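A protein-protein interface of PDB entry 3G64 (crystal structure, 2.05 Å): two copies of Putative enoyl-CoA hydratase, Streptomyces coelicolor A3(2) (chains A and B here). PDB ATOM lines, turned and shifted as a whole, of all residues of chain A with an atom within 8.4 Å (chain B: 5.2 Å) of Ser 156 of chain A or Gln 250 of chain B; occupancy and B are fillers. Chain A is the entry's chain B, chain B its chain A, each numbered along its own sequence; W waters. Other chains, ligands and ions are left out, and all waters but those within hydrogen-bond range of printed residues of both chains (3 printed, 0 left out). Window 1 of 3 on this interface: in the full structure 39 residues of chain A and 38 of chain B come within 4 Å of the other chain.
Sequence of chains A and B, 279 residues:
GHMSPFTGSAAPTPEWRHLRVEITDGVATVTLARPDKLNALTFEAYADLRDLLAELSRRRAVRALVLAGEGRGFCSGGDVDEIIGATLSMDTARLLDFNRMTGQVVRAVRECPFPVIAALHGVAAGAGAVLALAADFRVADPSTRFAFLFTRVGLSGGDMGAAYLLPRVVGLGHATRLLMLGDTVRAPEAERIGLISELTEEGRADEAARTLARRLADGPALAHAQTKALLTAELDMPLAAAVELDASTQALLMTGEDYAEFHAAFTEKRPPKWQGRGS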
ATOM      1  N   THR A  87       3.668  -8.224  21.242  1.00  0.00           N
ATOM      2  CA  THR A  87       2.604  -7.244  20.979  1.00  0.00           C
ATOM      3  C   THR A  87       3.157  -5.829  20.987  1.00  0.00           C
ATOM      4  O   THR A  87       2.607  -4.924  20.343  1.00  0.00           O
ATOM      5  CB  THR A  87       1.401  -7.355  21.962  1.00  0.00           C
ATOM      6  OG1 THR A  87       1.855  -7.246  23.321  1.00  0.00           O
ATOM      7  CG2 THR A  87       0.665  -8.669  21.762  1.00  0.00           C
ATOM      8  N   LEU A  95      -2.884  -5.309  16.694  1.00  0.00           N
ATOM      9  CA  LEU A  95      -3.299  -5.224  18.087  1.00  0.00           C
ATOM     10  C   LEU A  95      -4.811  -5.496  18.210  1.00  0.00           C
ATOM     11  O   LEU A  95      -5.248  -6.258  19.079  1.00  0.00           O
ATOM     12  CB  LEU A  95      -2.950  -3.858  18.682  1.00  0.00           C
ATOM     13  CG  LEU A  95      -1.465  -3.609  18.943  1.00  0.00           C
ATOM     14  CD1 LEU A  95      -1.221  -2.193  19.424  1.00  0.00           C
ATOM     15  CD2 LEU A  95      -0.869  -4.642  19.915  1.00  0.00           C
ATOM     16  N   LEU A  96      -5.601  -4.898  17.324  1.00  0.00           N
ATOM     17  CA  LEU A  96      -7.046  -5.123  17.338  1.00  0.00           C
ATOM     18  C   LEU A  96      -7.356  -6.588  16.991  1.00  0.00           C
ATOM     19  O   LEU A  96      -8.160  -7.247  17.668  1.00  0.00           O
ATOM     20  CB  LEU A  96      -7.760  -4.174  16.363  1.00  0.00           C
ATOM     21  CG  LEU A  96      -9.303  -4.276  16.328  1.00  0.00           C
ATOM     22  CD1 LEU A  96      -9.881  -3.926  17.701  1.00  0.00           C
ATOM     23  CD2 LEU A  96      -9.901  -3.392  15.236  1.00  0.00           C
ATOM     24  N   PHE A  98      -5.539  -9.219  17.407  1.00  0.00           N
ATOM     25  CA  PHE A  98      -5.196 -10.138  18.496  1.00  0.00           C
ATOM     26  C   PHE A  98      -6.293 -10.153  19.557  1.00  0.00           C
ATOM     27  O   PHE A  98      -6.752 -11.221  19.994  1.00  0.00           O
ATOM     28  CB  PHE A  98      -3.874  -9.767  19.171  1.00  0.00           C
ATOM     29  CG  PHE A  98      -3.621 -10.546  20.442  1.00  0.00           C
ATOM     30  CD1 PHE A  98      -3.362 -11.911  20.387  1.00  0.00           C
ATOM     31  CD2 PHE A  98      -3.678  -9.932  21.681  1.00  0.00           C
ATOM     32  CE1 PHE A  98      -3.149 -12.650  21.538  1.00  0.00           C
ATOM     33  CE2 PHE A  98      -3.461 -10.670  22.854  1.00  0.00           C
ATOM     34  CZ  PHE A  98      -3.202 -12.040  22.770  1.00  0.00           C
ATOM     35  N   ASN A  99      -6.696  -8.961  19.978  1.00  0.00           N
ATOM     36  CA  ASN A  99      -7.661  -8.849  21.067  1.00  0.00           C
ATOM     37  C   ASN A  99      -9.055  -9.271  20.619  1.00  0.00           C
ATOM     38  O   ASN A  99      -9.821  -9.799  21.415  1.00  0.00           O
ATOM     39  CB  ASN A  99      -7.629  -7.458  21.666  1.00  0.00           C
ATOM     40  CG  ASN A  99      -6.346  -7.196  22.409  1.00  0.00           C
ATOM     41  OD1 ASN A  99      -5.494  -6.425  21.964  1.00  0.00           O
ATOM     42  ND2 ASN A  99      -6.177  -7.874  23.525  1.00  0.00           N
ATOM     43  N   ARG A 100      -9.356  -9.107  19.336  1.00  0.00           N
ATOM     44  CA  ARG A 100     -10.555  -9.730  18.805  1.00  0.00           C
ATOM     45  C   ARG A 100     -10.478 -11.260  18.846  1.00  0.00           C
ATOM     46  O   ARG A 100     -11.458 -11.925  19.215  1.00  0.00           O
ATOM     47  CB  ARG A 100     -10.862  -9.263  17.392  1.00  0.00           C
ATOM     48  CG  ARG A 100     -12.178  -9.837  16.867  1.00  0.00           C
ATOM     49  CD  ARG A 100     -12.632  -9.153  15.571  1.00  0.00           C
ATOM     50  NE  ARG A 100     -13.227  -7.840  15.825  1.00  0.00           N
ATOM     51  CZ  ARG A 100     -12.833  -6.713  15.232  1.00  0.00           C
ATOM     52  NH1 ARG A 100     -11.833  -6.752  14.337  1.00  0.00           N
ATOM     53  NH2 ARG A 100     -13.444  -5.554  15.519  1.00  0.00           N
ATOM     54  N   THR A 102      -8.882 -13.285  20.865  1.00  0.00           N
ATOM     55  CA  THR A 102      -9.023 -13.864  22.194  1.00  0.00           C
ATOM     56  C   THR A 102     -10.489 -13.839  22.642  1.00  0.00           C
ATOM     57  O   THR A 102     -11.004 -14.827  23.181  1.00  0.00           O
ATOM     58  CB  THR A 102      -8.118 -13.156  23.229  1.00  0.00           C
ATOM     59  OG1 THR A 102      -8.380 -11.758  23.184  1.00  0.00           O
ATOM     60  CG2 THR A 102      -6.620 -13.412  22.902  1.00  0.00           C
ATOM     61  N   PHE A 148      -7.439 -13.086  38.117  1.00  0.00           N
ATOM     62  CA  PHE A 148      -7.780 -12.249  36.956  1.00  0.00           C
ATOM     63  C   PHE A 148      -6.839 -11.052  36.972  1.00  0.00           C
ATOM     64  O   PHE A 148      -7.223  -9.967  37.381  1.00  0.00           O
ATOM     65  CB  PHE A 148      -9.273 -11.798  37.012  1.00  0.00           C
ATOM     66  CG  PHE A 148     -10.235 -12.949  36.971  1.00  0.00           C
ATOM     67  CD1 PHE A 148     -10.750 -13.398  35.749  1.00  0.00           C
ATOM     68  CD2 PHE A 148     -10.586 -13.616  38.137  1.00  0.00           C
ATOM     69  CE1 PHE A 148     -11.607 -14.484  35.695  1.00  0.00           C
ATOM     70  CE2 PHE A 148     -11.444 -14.709  38.098  1.00  0.00           C
ATOM     71  CZ  PHE A 148     -11.950 -15.152  36.881  1.00  0.00           C
ATOM     72  N   LEU A 149      -5.607 -11.239  36.516  1.00  0.00           N
ATOM     73  CA  LEU A 149      -4.558 -10.260  36.818  1.00  0.00           C
ATOM     74  C   LEU A 149      -4.172  -9.310  35.673  1.00  0.00           C
ATOM     75  O   LEU A 149      -3.052  -8.784  35.619  1.00  0.00           O
ATOM     76  CB  LEU A 149      -3.325 -10.976  37.380  1.00  0.00           C
ATOM     77  CG  LEU A 149      -2.982 -12.257  36.631  1.00  0.00           C
ATOM     78  CD1 LEU A 149      -2.543 -11.913  35.223  1.00  0.00           C
ATOM     79  CD2 LEU A 149      -1.894 -13.015  37.392  1.00  0.00           C
ATOM     80  N   PHE A 150      -5.113  -9.060  34.780  1.00  0.00           N
ATOM     81  CA  PHE A 150      -4.884  -8.104  33.704  1.00  0.00           C
ATOM     82  C   PHE A 150      -4.337  -6.734  34.119  1.00  0.00           C
ATOM     83  O   PHE A 150      -3.425  -6.204  33.468  1.00  0.00           O
ATOM     84  CB  PHE A 150      -6.158  -7.988  32.885  1.00  0.00           C
ATOM     85  CG  PHE A 150      -6.643  -9.320  32.397  1.00  0.00           C
ATOM     86  CD1 PHE A 150      -5.939  -9.994  31.416  1.00  0.00           C
ATOM     87  CD2 PHE A 150      -7.757  -9.926  32.973  1.00  0.00           C
ATOM     88  CE1 PHE A 150      -6.354 -11.235  30.954  1.00  0.00           C
ATOM     89  CE2 PHE A 150      -8.187 -11.167  32.529  1.00  0.00           C
ATOM     90  CZ  PHE A 150      -7.475 -11.831  31.506  1.00  0.00           C
ATOM     91  N   THR A 151      -4.875  -6.154  35.189  1.00  0.00           N
ATOM     92  CA  THR A 151      -4.426  -4.833  35.603  1.00  0.00           C
ATOM     93  C   THR A 151      -2.965  -4.898  36.087  1.00  0.00           C
ATOM     94  O   THR A 151      -2.284  -3.875  36.141  1.00  0.00           O
ATOM     95  CB  THR A 151      -5.329  -4.202  36.700  1.00  0.00           C
ATOM     96  OG1 THR A 151      -5.432  -5.085  37.825  1.00  0.00           O
ATOM     97  CG2 THR A 151      -6.741  -3.905  36.140  1.00  0.00           C
ATOM     98  N   ARG A 152      -2.503  -6.095  36.443  1.00  0.00           N
ATOM     99  CA  ARG A 152      -1.104  -6.279  36.862  1.00  0.00           C
ATOM    100  C   ARG A 152      -0.166  -6.045  35.685  1.00  0.00           C
ATOM    101  O   ARG A 152       1.017  -5.805  35.886  1.00  0.00           O
ATOM    102  CB  ARG A 152      -0.833  -7.683  37.407  1.00  0.00           C
ATOM    103  CG  ARG A 152      -1.618  -8.075  38.653  1.00  0.00           C
ATOM    104  CD  ARG A 152      -1.509  -7.071  39.781  1.00  0.00           C
ATOM    105  NE  ARG A 152      -2.312  -7.494  40.929  1.00  0.00           N
ATOM    106  CZ  ARG A 152      -1.842  -8.198  41.958  1.00  0.00           C
ATOM    107  NH1 ARG A 152      -0.557  -8.551  41.989  1.00  0.00           N
ATOM    108  NH2 ARG A 152      -2.650  -8.556  42.954  1.00  0.00           N
ATOM    109  N   VAL A 153      -0.673  -6.149  34.454  1.00  0.00           N
ATOM    110  CA  VAL A 153       0.170  -5.900  33.291  1.00  0.00           C
ATOM    111  C   VAL A 153      -0.192  -4.599  32.595  1.00  0.00           C
ATOM    112  O   VAL A 153       0.283  -4.326  31.499  1.00  0.00           O
ATOM    113  CB  VAL A 153       0.173  -7.070  32.278  1.00  0.00           C
ATOM    114  CG1 VAL A 153       0.491  -8.390  32.994  1.00  0.00           C
ATOM    115  CG2 VAL A 153      -1.142  -7.137  31.523  1.00  0.00           C
ATOM    116  N   GLY A 154      -1.008  -3.785  33.261  1.00  0.00           N
ATOM    117  CA  GLY A 154      -1.383  -2.481  32.744  1.00  0.00           C
ATOM    118  C   GLY A 154      -2.496  -2.511  31.706  1.00  0.00           C
ATOM    119  O   GLY A 154      -2.664  -1.560  30.950  1.00  0.00           O
ATOM    120  N   LEU A 155      -3.228  -3.619  31.644  1.00  0.00           N
ATOM    121  CA  LEU A 155      -4.402  -3.735  30.768  1.00  0.00           C
ATOM    122  C   LEU A 155      -5.693  -3.720  31.619  1.00  0.00           C
ATOM    123  O   LEU A 155      -5.620  -3.813  32.833  1.00  0.00           O
ATOM    124  CB  LEU A 155      -4.322  -5.019  29.943  1.00  0.00           C
ATOM    125  CG  LEU A 155      -3.165  -5.131  28.938  1.00  0.00           C
ATOM    126  CD1 LEU A 155      -3.307  -6.404  28.120  1.00  0.00           C
ATOM    127  CD2 LEU A 155      -3.111  -3.921  28.014  1.00  0.00           C
ATOM    128  N   SER A 156      -6.882  -3.610  31.019  1.00  0.00           N
ATOM    129  CA  SER A 156      -8.046  -3.579  31.896  1.00  0.00           C
ATOM    130  C   SER A 156      -8.531  -5.002  32.160  1.00  0.00           C
ATOM    131  O   SER A 156      -8.227  -5.908  31.384  1.00  0.00           O
ATOM    132  CB  SER A 156      -9.183  -2.746  31.293  1.00  0.00           C
ATOM    133  OG  SER A 156      -9.934  -3.561  30.425  1.00  0.00           O
ATOM    134  N   GLY A 157      -9.295  -5.183  33.247  1.00  0.00           N
ATOM    135  CA  GLY A 157      -9.965  -6.447  33.546  1.00  0.00           C
ATOM    136  C   GLY A 157     -11.085  -6.864  32.586  1.00  0.00           C
ATOM    137  O   GLY A 157     -11.630  -7.958  32.694  1.00  0.00           O
ATOM    138  N   GLY A 158     -11.425  -6.004  31.633  1.00  0.00           N
ATOM    139  CA  GLY A 158     -12.355  -6.383  30.584  1.00  0.00           C
ATOM    140  C   GLY A 158     -11.590  -7.032  29.444  1.00  0.00           C
ATOM    141  O   GLY A 158     -11.608  -6.554  28.320  1.00  0.00           O
ATOM    142  N   ASP A 159     -10.842  -8.086  29.752  1.00  0.00           N
ATOM    143  CA  ASP A 159     -10.096  -8.782  28.723  1.00  0.00           C
ATOM    144  C   ASP A 159     -10.932  -9.970  28.287  1.00  0.00           C
ATOM    145  O   ASP A 159     -11.396 -10.749  29.138  1.00  0.00           O
ATOM    146  CB  ASP A 159      -8.736  -9.263  29.284  1.00  0.00           C
ATOM    147  CG  ASP A 159      -7.761  -9.712  28.180  1.00  0.00           C
ATOM    148  OD1 ASP A 159      -7.061  -8.847  27.593  1.00  0.00           O
ATOM    149  OD2 ASP A 159      -7.691 -10.938  27.923  1.00  0.00           O
ATOM    150  N   MET A 160     -11.096 -10.107  26.972  1.00  0.00           N
ATOM    151  CA  MET A 160     -11.712 -11.277  26.330  1.00  0.00           C
ATOM    152  C   MET A 160     -13.002 -11.772  27.016  1.00  0.00           C
ATOM    153  O   MET A 160     -13.250 -12.970  27.127  1.00  0.00           O
ATOM    154  CB  MET A 160     -10.692 -12.423  26.138  1.00  0.00           C
ATOM    155  CG  MET A 160     -10.059 -12.928  27.399  1.00  0.00           C
ATOM    156  SD  MET A 160      -8.420 -14.010  27.124  1.00  0.00           S
ATOM    157  CE  MET A 160      -9.293 -15.637  26.429  1.00  0.00           C
ATOM    158  N   GLY A 161     -13.835 -10.836  27.446  1.00  0.00           N
ATOM    159  CA  GLY A 161     -15.152 -11.174  27.961  1.00  0.00           C
ATOM    160  C   GLY A 161     -15.234 -11.300  29.481  1.00  0.00           C
ATOM    161  O   GLY A 161     -16.318 -11.535  30.018  1.00  0.00           O
ATOM    162  N   ALA A 162     -14.105 -11.148  30.176  1.00  0.00           N
ATOM    163  CA  ALA A 162     -14.114 -11.307  31.628  1.00  0.00           C
ATOM    164  C   ALA A 162     -15.086 -10.367  32.341  1.00  0.00           C
ATOM    165  O   ALA A 162     -15.746 -10.775  33.302  1.00  0.00           O
ATOM    166  CB  ALA A 162     -12.685 -11.165  32.229  1.00  0.00           C
ATOM    167  N   ALA A 163     -15.165  -9.112  31.895  1.00  0.00           N
ATOM    168  CA  ALA A 163     -16.059  -8.128  32.531  1.00  0.00           C
ATOM    169  C   ALA A 163     -17.551  -8.404  32.277  1.00  0.00           C
ATOM    170  O   ALA A 163     -18.421  -8.009  33.071  1.00  0.00           O
ATOM    171  CB  ALA A 163     -15.715  -6.699  32.097  1.00  0.00           C
ATOM    172  N   LEU A 179     -11.457  -8.322  39.441  1.00  0.00           N
ATOM    173  CA  LEU A 179     -10.909  -7.859  38.167  1.00  0.00           C
ATOM    174  C   LEU A 179     -10.075  -6.621  38.384  1.00  0.00           C
ATOM    175  O   LEU A 179      -9.152  -6.351  37.645  1.00  0.00           O
ATOM    176  CB  LEU A 179     -12.020  -7.557  37.135  1.00  0.00           C
ATOM    177  CG  LEU A 179     -12.774  -8.761  36.552  1.00  0.00           C
ATOM    178  CD1 LEU A 179     -13.844  -8.333  35.575  1.00  0.00           C
ATOM    179  CD2 LEU A 179     -11.813  -9.682  35.875  1.00  0.00           C
ATOM    180  N   MET A 180     -10.405  -5.835  39.389  1.00  0.00           N
ATOM    181  CA  MET A 180      -9.600  -4.637  39.573  1.00  0.00           C
ATOM    182  C   MET A 180      -8.281  -4.787  40.316  1.00  0.00           C
ATOM    183  O   MET A 180      -7.284  -4.155  39.924  1.00  0.00           O
ATOM    184  CB  MET A 180     -10.374  -3.486  40.138  1.00  0.00           C
ATOM    185  CG  MET A 180     -10.341  -2.406  39.111  1.00  0.00           C
ATOM    186  SD  MET A 180     -10.672  -0.766  39.942  1.00  0.00           S
ATOM    187  CE  MET A 180     -12.613  -0.924  39.768  1.00  0.00           C
ATOM    188  N   ALA B 223      -5.722   1.689  33.186  1.00  0.00           N
ATOM    189  CA  ALA B 223      -6.176   0.306  33.311  1.00  0.00           C
ATOM    190  C   ALA B 223      -7.315   0.129  34.332  1.00  0.00           C
ATOM    191  O   ALA B 223      -8.299  -0.584  34.041  1.00  0.00           O
ATOM    192  CB  ALA B 223      -5.001  -0.631  33.651  1.00  0.00           C
ATOM    193  N   GLN B 226     -10.651   1.999  33.012  1.00  0.00           N
ATOM    194  CA  GLN B 226     -11.252   1.202  31.958  1.00  0.00           C
ATOM    195  C   GLN B 226     -11.820  -0.124  32.461  1.00  0.00           C
ATOM    196  O   GLN B 226     -12.764  -0.638  31.887  1.00  0.00           O
ATOM    197  CB  GLN B 226     -10.284   0.977  30.790  1.00  0.00           C
ATOM    198  CG  GLN B 226     -10.067   2.235  29.935  1.00  0.00           C
ATOM    199  CD  GLN B 226     -11.396   2.856  29.458  1.00  0.00           C
ATOM    200  OE1 GLN B 226     -11.898   3.796  30.060  1.00  0.00           O
ATOM    201  NE2 GLN B 226     -11.964   2.307  28.384  1.00  0.00           N
ATOM    202  N   THR B 227     -11.256  -0.687  33.516  1.00  0.00           N
ATOM    203  CA  THR B 227     -11.850  -1.892  34.095  1.00  0.00           C
ATOM    204  C   THR B 227     -13.265  -1.567  34.610  1.00  0.00           C
ATOM    205  O   THR B 227     -14.222  -2.331  34.393  1.00  0.00           O
ATOM    206  CB  THR B 227     -10.993  -2.452  35.282  1.00  0.00           C
ATOM    207  OG1 THR B 227      -9.698  -2.853  34.793  1.00  0.00           O
ATOM    208  CG2 THR B 227     -11.685  -3.667  35.928  1.00  0.00           C
ATOM    209  N   LEU B 230     -15.716  -0.854  31.691  1.00  0.00           N
ATOM    210  CA  LEU B 230     -16.200  -2.043  30.965  1.00  0.00           C
ATOM    211  C   LEU B 230     -17.170  -2.896  31.789  1.00  0.00           C
ATOM    212  O   LEU B 230     -18.124  -3.442  31.252  1.00  0.00           O
ATOM    213  CB  LEU B 230     -15.036  -2.887  30.404  1.00  0.00           C
ATOM    214  CG  LEU B 230     -14.657  -2.477  28.961  1.00  0.00           C
ATOM    215  CD1 LEU B 230     -14.394  -0.971  28.829  1.00  0.00           C
ATOM    216  CD2 LEU B 230     -13.463  -3.250  28.480  1.00  0.00           C
ATOM    217  N   LEU B 245     -16.026  -4.308  22.561  1.00  0.00           N
ATOM    218  CA  LEU B 245     -15.553  -3.246  23.462  1.00  0.00           C
ATOM    219  C   LEU B 245     -14.220  -3.648  24.129  1.00  0.00           C
ATOM    220  O   LEU B 245     -13.305  -2.844  24.260  1.00  0.00           O
ATOM    221  CB  LEU B 245     -16.607  -2.931  24.546  1.00  0.00           C
ATOM    222  CG  LEU B 245     -16.300  -1.864  25.615  1.00  0.00           C
ATOM    223  CD1 LEU B 245     -15.910  -0.543  24.978  1.00  0.00           C
ATOM    224  CD2 LEU B 245     -17.499  -1.646  26.602  1.00  0.00           C
ATOM    225  N   ASP B 246     -14.158  -4.887  24.585  1.00  0.00           N
ATOM    226  CA  ASP B 246     -12.911  -5.446  25.126  1.00  0.00           C
ATOM    227  C   ASP B 246     -11.767  -5.330  24.126  1.00  0.00           C
ATOM    228  O   ASP B 246     -10.687  -4.855  24.465  1.00  0.00           O
ATOM    229  CB  ASP B 246     -13.083  -6.917  25.432  1.00  0.00           C
ATOM    230  CG  ASP B 246     -13.990  -7.162  26.588  1.00  0.00           C
ATOM    231  OD1 ASP B 246     -14.387  -6.180  27.264  1.00  0.00           O
ATOM    232  OD2 ASP B 246     -14.309  -8.347  26.822  1.00  0.00           O
ATOM    233  N   ALA B 247     -12.016  -5.794  22.900  1.00  0.00           N
ATOM    234  CA  ALA B 247     -11.021  -5.770  21.832  1.00  0.00           C
ATOM    235  C   ALA B 247     -10.498  -4.360  21.586  1.00  0.00           C
ATOM    236  O   ALA B 247      -9.295  -4.140  21.589  1.00  0.00           O
ATOM    237  CB  ALA B 247     -11.604  -6.364  20.531  1.00  0.00           C
ATOM    238  N   SER B 248     -11.405  -3.411  21.364  1.00  0.00           N
ATOM    239  CA  SER B 248     -10.998  -2.018  21.184  1.00  0.00           C
ATOM    240  C   SER B 248     -10.199  -1.482  22.372  1.00  0.00           C
ATOM    241  O   SER B 248      -9.173  -0.843  22.197  1.00  0.00           O
ATOM    242  CB  SER B 248     -12.227  -1.120  20.959  1.00  0.00           C
ATOM    243  OG  SER B 248     -12.708  -1.290  19.638  1.00  0.00           O
ATOM    244  N   THR B 249     -10.699  -1.719  23.579  1.00  0.00           N
ATOM    245  CA  THR B 249     -10.099  -1.151  24.775  1.00  0.00           C
ATOM    246  C   THR B 249      -8.706  -1.763  25.057  1.00  0.00           C
ATOM    247  O   THR B 249      -7.759  -1.038  25.380  1.00  0.00           O
ATOM    248  CB  THR B 249     -11.031  -1.376  26.003  1.00  0.00           C
ATOM    249  OG1 THR B 249     -12.299  -0.704  25.795  1.00  0.00           O
ATOM    250  CG2 THR B 249     -10.404  -0.873  27.252  1.00  0.00           C
ATOM    251  N   GLN B 250      -8.610  -3.092  24.992  1.00  0.00           N
ATOM    252  CA  GLN B 250      -7.347  -3.781  25.265  1.00  0.00           C
ATOM    253  C   GLN B 250      -6.316  -3.366  24.212  1.00  0.00           C
ATOM    254  O   GLN B 250      -5.186  -3.046  24.543  1.00  0.00           O
ATOM    255  CB  GLN B 250      -7.523  -5.302  25.279  1.00  0.00           C
ATOM    256  CG  GLN B 250      -8.295  -5.881  26.461  1.00  0.00           C
ATOM    257  CD  GLN B 250      -7.778  -5.432  27.851  1.00  0.00           C
ATOM    258  OE1 GLN B 250      -7.763  -4.243  28.177  1.00  0.00           O
ATOM    259  NE2 GLN B 250      -7.402  -6.396  28.676  1.00  0.00           N
ATOM    260  N   ALA B 251      -6.712  -3.339  22.943  1.00  0.00           N
ATOM    261  CA  ALA B 251      -5.784  -2.891  21.916  1.00  0.00           C
ATOM    262  C   ALA B 251      -5.315  -1.457  22.206  1.00  0.00           C
ATOM    263  O   ALA B 251      -4.122  -1.160  22.107  1.00  0.00           O
ATOM    264  CB  ALA B 251      -6.382  -3.036  20.518  1.00  0.00           C
ATOM    265  N   LEU B 252      -6.228  -0.569  22.598  1.00  0.00           N
ATOM    266  CA  LEU B 252      -5.815   0.792  22.947  1.00  0.00           C
ATOM    267  C   LEU B 252      -4.800   0.790  24.092  1.00  0.00           C
ATOM    268  O   LEU B 252      -3.799   1.524  24.071  1.00  0.00           O
ATOM    269  CB  LEU B 252      -7.015   1.672  23.329  1.00  0.00           C
ATOM    270  CG  LEU B 252      -6.703   3.059  23.905  1.00  0.00           C
ATOM    271  CD1 LEU B 252      -6.142   3.932  22.821  1.00  0.00           C
ATOM    272  CD2 LEU B 252      -7.974   3.715  24.473  1.00  0.00           C
ATOM    273  N   LEU B 253      -5.053  -0.025  25.104  1.00  0.00           N
ATOM    274  CA  LEU B 253      -4.207   0.017  26.284  1.00  0.00           C
ATOM    275  C   LEU B 253      -2.822  -0.590  25.967  1.00  0.00           C
ATOM    276  O   LEU B 253      -1.812  -0.238  26.587  1.00  0.00           O
ATOM    277  CB  LEU B 253      -4.874  -0.699  27.473  1.00  0.00           C
ATOM    278  CG  LEU B 253      -6.099   0.019  28.091  1.00  0.00           C
ATOM    279  CD1 LEU B 253      -6.721  -0.779  29.220  1.00  0.00           C
ATOM    280  CD2 LEU B 253      -5.699   1.357  28.594  1.00  0.00           C
ATOM    281  N   MET B 254      -2.796  -1.504  25.009  1.00  0.00           N
ATOM    282  CA  MET B 254      -1.543  -2.078  24.541  1.00  0.00           C
ATOM    283  C   MET B 254      -0.641  -1.054  23.821  1.00  0.00           C
ATOM    284  O   MET B 254       0.529  -1.346  23.568  1.00  0.00           O
ATOM    285  CB  MET B 254      -1.797  -3.296  23.658  1.00  0.00           C
ATOM    286  CG  MET B 254      -2.098  -4.548  24.438  1.00  0.00           C
ATOM    287  SD  MET B 254      -2.178  -6.085  23.239  1.00  0.00           S
ATOM    288  CE  MET B 254      -2.614  -7.445  24.563  1.00  0.00           C
HETATM  289  O   HOH W   1      -1.265   0.459  29.258  1.00  0.00           O
HETATM  290  O   HOH W   2     -15.468  -8.301  29.218  1.00  0.00           O
HETATM  291  O   HOH W   3     -14.080  -3.459  18.183  1.00  0.00           O
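OG1 of Thr 227 of chain B lies within hydrogen-bond range of N of Gly 157 of chain A (2.8 Å).
OD1 of Asp 246 of chain B lies close to O of Gly 158 of chain A.
The side-chain amide oxygen (OD1) of Asn 99 of chain A lies close to the side-chain sulfur (SD) of Met 254 of chain B, 3.6 Å away.
The backbone NH (N) of Gly 161 of chain A is in hydrogen-bond range of the side-chain carboxylate (OD2) of Asp 246 of chain B (2.6 Å).
NE2 of Gln 250 of chain B lies within hydrogen-bond range of OD1 of Asp 159 of chain A (2.7 Å).
The backbone NH (N) of Ala 251 of chain B is in hydrogen-bond range of the side-chain amide oxygen (OD1) of Asn 99 of chain A.
The side-chain amide nitrogen (NE2) of Gln 250 of chain B sits at hydrogen-bond distance from the backbone carbonyl oxygen (O) of Ser 156 of chain A (2.9 Å).
O of Met 180 of chain A is in hydrogen-bond range of OG1 of Thr 151 of chain A, 2.9 Å away.
N of Leu 155 of chain A is in hydrogen-bond range of O of Phe 150 of chain A, at 3.2 Å.
The side-chain hydroxyl (OG1) of Thr 227 of chain B is in hydrogen-bond range of the backbone carbonyl oxygen (O) of Ala 223 of chain B (2.8 Å).
The side-chain hydroxyl of Ser 156 of chain A is in hydrogen-bond range of the backbone NH of Gly 158 of chain A (3.1 Å).
The backbone carbonyl oxygen (O) of Asn 99 of chain A is in hydrogen-bond range of the side-chain hydroxyl (OG1) of Thr 102 of chain A (3.0 Å).
The side-chain amide oxygen of Asn 99 of chain A lies close to the backbone carbonyl oxygen of Leu 95 of chain A (2.9 Å).
O of Leu 95 of chain A touches CB of Ala 251 of chain B (3.7 Å).
Leu 96 of chain A touches Ala 251 of chain B.
Met 254 of chain B touches Phe 98 of chain A.
CB of Ala 247 of chain B touches N of Arg 100 of chain A, at 3.7 Å.
Gly 154 of chain A touches Ala 223 of chain B (C to CB, 3.7 Å).
Leu 155 of chain A touches Ala 223 of chain B.
CB of Leu 155 of chain A touches NE2 of Gln 250 of chain B (3.6 Å).
Gly 158 of chain A touches Leu 230 of chain B (O to CD2, 3.8 Å).
Met 160 of chain A touches Asp 246 of chain B.
Thr 227 of chain B touches Met 180 of chain A (CG2 to CG, 3.7 Å).
Of the printed residues of chain B, Arg 100 of chain A touches Ala 247 (3.7 Å).
Phe 148 of chain A touches none of the printed residues of chain B.
Printed residues of chain B within 4 Å of Gly 157 of chain A: Thr 227.
Of the printed residues of chain A, Gln 226 of chain B touches Ser 156.
Ser 248 of chain B touches none of the printed residues of chain A.
Of chain A, only Asn 99 (3.4 Å), Leu 155 (3.6 Å), Ser 156 (2.9 Å), Gly 158 (3.9 Å) and Asp 159 (2.7 Å) come within 4 Å of Gln 250 of chain B.
Of the printed residues of chain A, Met 254 of chain B touches Leu 95, Phe 98, Asn 99 and Leu 155.
The nearest residue of chain A that does not touch Gln 250 of chain B is Phe 150 of chain A (4.7 Å).
The nearest printed residue of chain B that does not touch Gly 161 of chain A is Ala 247 of chain B (7.0 Å).
Of the 14 printed residues of chain B, 10 touch a printed residue of chain A.
Hydrophobic or aromatic side chains of chain B that line the printed part of chain A: Ala 223, Leu 230, Ala 247, Ala 251, Leu 253 and Met 254.
Among the printed residues, no Asp or Glu carboxylate lies within 4 Å of a Lys or Arg side-chain nitrogen of the other chain.
No position is printed for both chains.
Water W2 lies within hydrogen-bond range of the side-chain carboxylate (OD2) of Asp 246 of chain B, the backbone NH (N) of Ala 163 of chain A, the backbone NH (N) of Ala 162 of chain A and the backbone carbonyl oxygen (O) of Gly 161 of chain A.
Water W1 bridges O of Leu 253 of chain B (2.8 Å) and O of Gly 154 of chain A (3.0 Å).
Water W3 lies within hydrogen-bond range of the side-chain hydroxyl of Ser 248 of chain B and the guanidinium group of Arg 100 of chain A.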
